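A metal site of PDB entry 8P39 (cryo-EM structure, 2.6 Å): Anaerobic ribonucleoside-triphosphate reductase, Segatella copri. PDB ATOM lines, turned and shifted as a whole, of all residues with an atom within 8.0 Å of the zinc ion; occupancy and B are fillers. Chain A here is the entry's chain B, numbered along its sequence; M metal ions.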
ATOM      1  N   ARG A 683     -31.479 -13.137  28.722  1.00  0.00           N
ATOM      2  CA  ARG A 683     -30.750 -12.162  29.521  1.00  0.00           C
ATOM      3  C   ARG A 683     -29.275 -12.499  29.574  1.00  0.00           C
ATOM      4  O   ARG A 683     -28.837 -13.583  29.192  1.00  0.00           O
ATOM      5  CB  ARG A 683     -31.326 -12.076  30.935  1.00  0.00           C
ATOM      6  CG  ARG A 683     -32.346 -10.978  31.138  1.00  0.00           C
ATOM      7  CD  ARG A 683     -32.645 -10.773  32.610  1.00  0.00           C
ATOM      8  NE  ARG A 683     -33.408  -9.558  32.862  1.00  0.00           N
ATOM      9  CZ  ARG A 683     -32.880  -8.367  33.071  1.00  0.00           C
ATOM     10  NH1 ARG A 683     -31.562  -8.184  33.070  1.00  0.00           N
ATOM     11  NH2 ARG A 683     -33.676  -7.330  33.287  1.00  0.00           N
ATOM     12  N   CYS A 684     -28.498 -11.540  30.071  1.00  0.00           N
ATOM     13  CA  CYS A 684     -27.052 -11.703  30.251  1.00  0.00           C
ATOM     14  C   CYS A 684     -26.688 -11.214  31.639  1.00  0.00           C
ATOM     15  O   CYS A 684     -27.147 -10.146  32.065  1.00  0.00           O
ATOM     16  CB  CYS A 684     -26.276 -10.924  29.176  1.00  0.00           C
ATOM     17  SG  CYS A 684     -24.565 -10.542  29.612  1.00  0.00           S
ATOM     18  N   LEU A 685     -25.862 -11.987  32.347  1.00  0.00           N
ATOM     19  CA  LEU A 685     -25.442 -11.631  33.693  1.00  0.00           C
ATOM     20  C   LEU A 685     -24.278 -10.644  33.719  1.00  0.00           C
ATOM     21  O   LEU A 685     -23.877 -10.223  34.813  1.00  0.00           O
ATOM     22  CB  LEU A 685     -25.082 -12.890  34.480  1.00  0.00           C
ATOM     23  CG  LEU A 685     -26.196 -13.544  35.306  1.00  0.00           C
ATOM     24  CD1 LEU A 685     -27.324 -14.060  34.419  1.00  0.00           C
ATOM     25  CD2 LEU A 685     -25.638 -14.676  36.164  1.00  0.00           C
ATOM     26  N   ASP A 686     -23.734 -10.288  32.558  1.00  0.00           N
ATOM     27  CA  ASP A 686     -22.639  -9.332  32.504  1.00  0.00           C
ATOM     28  C   ASP A 686     -23.070  -8.039  31.825  1.00  0.00           C
ATOM     29  O   ASP A 686     -22.925  -6.952  32.393  1.00  0.00           O
ATOM     30  CB  ASP A 686     -21.436  -9.944  31.781  1.00  0.00           C
ATOM     31  CG  ASP A 686     -20.877 -11.163  32.491  1.00  0.00           C
ATOM     32  OD1 ASP A 686     -21.633 -12.147  32.668  1.00  0.00           O
ATOM     33  OD2 ASP A 686     -19.692 -11.137  32.877  1.00  0.00           O
ATOM     34  N   CYS A 687     -23.608  -8.147  30.606  1.00  0.00           N
ATOM     35  CA  CYS A 687     -24.037  -6.960  29.878  1.00  0.00           C
ATOM     36  C   CYS A 687     -25.480  -6.593  30.220  1.00  0.00           C
ATOM     37  O   CYS A 687     -25.814  -5.414  30.350  1.00  0.00           O
ATOM     38  CB  CYS A 687     -23.892  -7.190  28.372  1.00  0.00           C
ATOM     39  SG  CYS A 687     -22.263  -7.780  27.883  1.00  0.00           S
ATOM     40  N   GLY A 688     -26.339  -7.599  30.358  1.00  0.00           N
ATOM     41  CA  GLY A 688     -27.757  -7.377  30.562  1.00  0.00           C
ATOM     42  C   GLY A 688     -28.569  -7.262  29.291  1.00  0.00           C
ATOM     43  O   GLY A 688     -29.729  -6.853  29.359  1.00  0.00           O
ATOM     44  N   TYR A 689     -27.996  -7.620  28.158  1.00  0.00           N
ATOM     45  CA  TYR A 689     -28.668  -7.466  26.867  1.00  0.00           C
ATOM     46  C   TYR A 689     -29.780  -8.490  26.708  1.00  0.00           C
ATOM     47  O   TYR A 689     -29.689  -9.633  27.156  1.00  0.00           O
ATOM     48  CB  TYR A 689     -27.661  -7.613  25.727  1.00  0.00           C
ATOM     49  CG  TYR A 689     -28.255  -7.416  24.354  1.00  0.00           C
ATOM     50  CD1 TYR A 689     -28.488  -6.149  23.841  1.00  0.00           C
ATOM     51  CD2 TYR A 689     -28.589  -8.509  23.555  1.00  0.00           C
ATOM     52  CE1 TYR A 689     -29.020  -5.970  22.581  1.00  0.00           C
ATOM     53  CE2 TYR A 689     -29.129  -8.342  22.294  1.00  0.00           C
ATOM     54  CZ  TYR A 689     -29.345  -7.065  21.819  1.00  0.00           C
ATOM     55  OH  TYR A 689     -29.884  -6.898  20.557  1.00  0.00           O
ATOM     56  N   LEU A 696     -30.555 -18.508  23.137  1.00  0.00           N
ATOM     57  CA  LEU A 696     -29.275 -17.817  23.198  1.00  0.00           C
ATOM     58  C   LEU A 696     -28.414 -18.474  24.268  1.00  0.00           C
ATOM     59  O   LEU A 696     -28.910 -18.866  25.330  1.00  0.00           O
ATOM     60  CB  LEU A 696     -29.468 -16.326  23.516  1.00  0.00           C
ATOM     61  CG  LEU A 696     -28.242 -15.420  23.380  1.00  0.00           C
ATOM     62  CD1 LEU A 696     -27.743 -15.404  21.940  1.00  0.00           C
ATOM     63  CD2 LEU A 696     -28.554 -14.013  23.855  1.00  0.00           C
ATOM     64  N   VAL A 698     -24.534 -17.498  24.344  1.00  0.00           N
ATOM     65  CA  VAL A 698     -23.438 -16.574  24.586  1.00  0.00           C
ATOM     66  C   VAL A 698     -23.920 -15.171  24.222  1.00  0.00           C
ATOM     67  O   VAL A 698     -24.520 -14.977  23.151  1.00  0.00           O
ATOM     68  CB  VAL A 698     -22.165 -16.939  23.813  1.00  0.00           C
ATOM     69  CG1 VAL A 698     -21.488 -18.133  24.458  1.00  0.00           C
ATOM     70  CG2 VAL A 698     -22.494 -17.240  22.351  1.00  0.00           C
ATOM     71  N   CYS A 699     -23.683 -14.202  25.104  1.00  0.00           N
ATOM     72  CA  CYS A 699     -24.044 -12.820  24.843  1.00  0.00           C
ATOM     73  C   CYS A 699     -23.232 -12.282  23.671  1.00  0.00           C
ATOM     74  O   CYS A 699     -22.013 -12.485  23.615  1.00  0.00           O
ATOM     75  CB  CYS A 699     -23.825 -11.952  26.077  1.00  0.00           C
ATOM     76  SG  CYS A 699     -24.320 -10.230  25.879  1.00  0.00           S
ATOM     77  N   PRO A 700     -23.870 -11.618  22.695  1.00  0.00           N
ATOM     78  CA  PRO A 700     -23.127 -11.081  21.560  1.00  0.00           C
ATOM     79  C   PRO A 700     -22.062 -10.060  21.957  1.00  0.00           C
ATOM     80  O   PRO A 700     -21.017  -9.955  21.311  1.00  0.00           O
ATOM     81  CB  PRO A 700     -24.224 -10.437  20.689  1.00  0.00           C
ATOM     82  CG  PRO A 700     -25.356 -10.181  21.639  1.00  0.00           C
ATOM     83  CD  PRO A 700     -25.309 -11.294  22.630  1.00  0.00           C
ATOM     84  N   LYS A 701     -22.333  -9.307  23.022  1.00  0.00           N
ATOM     85  CA  LYS A 701     -21.412  -8.247  23.447  1.00  0.00           C
ATOM     86  C   LYS A 701     -20.255  -8.807  24.274  1.00  0.00           C
ATOM     87  O   LYS A 701     -19.095  -8.709  23.877  1.00  0.00           O
ATOM     88  CB  LYS A 701     -22.184  -7.175  24.226  1.00  0.00           C
ATOM     89  CG  LYS A 701     -23.314  -6.527  23.444  1.00  0.00           C
ATOM     90  CD  LYS A 701     -24.250  -5.762  24.365  1.00  0.00           C
ATOM     91  CE  LYS A 701     -23.511  -4.701  25.166  1.00  0.00           C
ATOM     92  NZ  LYS A 701     -24.421  -3.970  26.096  1.00  0.00           N
ATOM     93  N   CYS A 702     -20.574  -9.398  25.421  1.00  0.00           N
ATOM     94  CA  CYS A 702     -19.548  -9.852  26.360  1.00  0.00           C
ATOM     95  C   CYS A 702     -18.948 -11.189  25.944  1.00  0.00           C
ATOM     96  O   CYS A 702     -17.754 -11.283  25.647  1.00  0.00           O
ATOM     97  CB  CYS A 702     -20.126  -9.966  27.765  1.00  0.00           C
ATOM     98  SG  CYS A 702     -21.291 -11.330  27.954  1.00  0.00           S
ATOM     99  N   GLY A 703     -19.780 -12.230  25.928  1.00  0.00           N
ATOM    100  CA  GLY A 703     -19.298 -13.573  25.640  1.00  0.00           C
ATOM    101  C   GLY A 703     -19.578 -14.542  26.775  1.00  0.00           C
ATOM    102  O   GLY A 703     -19.194 -15.716  26.698  1.00  0.00           O
ATOM    103  N   SER A 704     -20.239 -14.058  27.822  1.00  0.00           N
ATOM    104  CA  SER A 704     -20.523 -14.901  28.982  1.00  0.00           C
ATOM    105  C   SER A 704     -21.474 -16.022  28.604  1.00  0.00           C
ATOM    106  O   SER A 704     -22.316 -15.893  27.708  1.00  0.00           O
ATOM    107  CB  SER A 704     -21.126 -14.059  30.107  1.00  0.00           C
ATOM    108  OG  SER A 704     -21.547 -14.872  31.189  1.00  0.00           O
ATOM    109  N   HIS A 705     -21.338 -17.153  29.298  1.00  0.00           N
ATOM    110  CA  HIS A 705     -22.156 -18.325  29.073  1.00  0.00           C
ATOM    111  C   HIS A 705     -23.371 -18.383  29.987  1.00  0.00           C
ATOM    112  O   HIS A 705     -24.131 -19.366  29.930  1.00  0.00           O
ATOM    113  CB  HIS A 705     -21.317 -19.598  29.238  1.00  0.00           C
ATOM    114  CG  HIS A 705     -21.197 -20.413  27.994  1.00  0.00           C
ATOM    115  ND1 HIS A 705     -20.243 -20.157  27.029  1.00  0.00           N
ATOM    116  CD2 HIS A 705     -21.908 -21.479  27.551  1.00  0.00           C
ATOM    117  CE1 HIS A 705     -20.369 -21.027  26.047  1.00  0.00           C
ATOM    118  NE2 HIS A 705     -21.366 -21.842  26.332  1.00  0.00           N
ATOM    119  N   HIS A 706     -23.575 -17.370  30.821  1.00  0.00           N
ATOM    120  CA  HIS A 706     -24.695 -17.348  31.750  1.00  0.00           C
ATOM    121  C   HIS A 706     -25.885 -16.611  31.125  1.00  0.00           C
ATOM    122  O   HIS A 706     -26.407 -15.640  31.664  1.00  0.00           O
ATOM    123  CB  HIS A 706     -24.284 -16.696  33.066  1.00  0.00           C
ATOM    124  CG  HIS A 706     -22.879 -17.018  33.488  1.00  0.00           C
ATOM    125  ND1 HIS A 706     -21.801 -16.246  33.120  1.00  0.00           N
ATOM    126  CD2 HIS A 706     -22.379 -18.033  34.235  1.00  0.00           C
ATOM    127  CE1 HIS A 706     -20.697 -16.763  33.620  1.00  0.00           C
ATOM    128  NE2 HIS A 706     -21.027 -17.846  34.303  1.00  0.00           N
ATOM    129  N   ILE A 707     -26.309 -17.110  29.963  1.00  0.00           N
ATOM    130  CA  ILE A 707     -27.433 -16.505  29.228  1.00  0.00           C
ATOM    131  C   ILE A 707     -28.693 -17.229  29.683  1.00  0.00           C
ATOM    132  O   ILE A 707     -28.994 -18.341  29.261  1.00  0.00           O
ATOM    133  CB  ILE A 707     -27.229 -16.578  27.716  1.00  0.00           C
ATOM    134  CG1 ILE A 707     -26.000 -15.772  27.305  1.00  0.00           C
ATOM    135  CG2 ILE A 707     -28.453 -16.054  27.001  1.00  0.00           C
ATOM    136  CD1 ILE A 707     -26.089 -14.307  27.643  1.00  0.00           C
HETATM  137 ZN    ZN M   1     -23.147  -9.934  27.860  1.00  0.00          ZN
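The backbone carbonyl oxygen (O) of Ser 704 is in hydrogen-bond range of the backbone NH (N) of Cys 699 (3.4 Å).
The backbone NH (N) of Gly 688 lies close to the side-chain sulfur (SG) of Cys 684 (3.5 Å).
The backbone NH of Lys 701 sits close to the side-chain sulfur of Cys 699 (3.6 Å).
SG of Cys 684 lies close to N of Asp 686.
The backbone NH (N) of Ser 704 sits close to the side-chain sulfur (SG) of Cys 702.
Of the 18 residues printed, 4 come within 4 Å of the zinc ion.
The nearest printed residue that does not touch the zinc ion is Asp 686 (4.3 Å).
The zinc ion is bound by the side-chain sulfur (SG) of Cys 699, at 2.3 Å.
SG of Cys 702 is bound to the zinc ion (2.3 Å).
SG of Cys 687 is bound to the zinc ion.
The side-chain sulfur (SG) of Cys 684 binds the zinc ion, at 2.3 Å.
The zinc ion has four donor atoms within binding distance.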
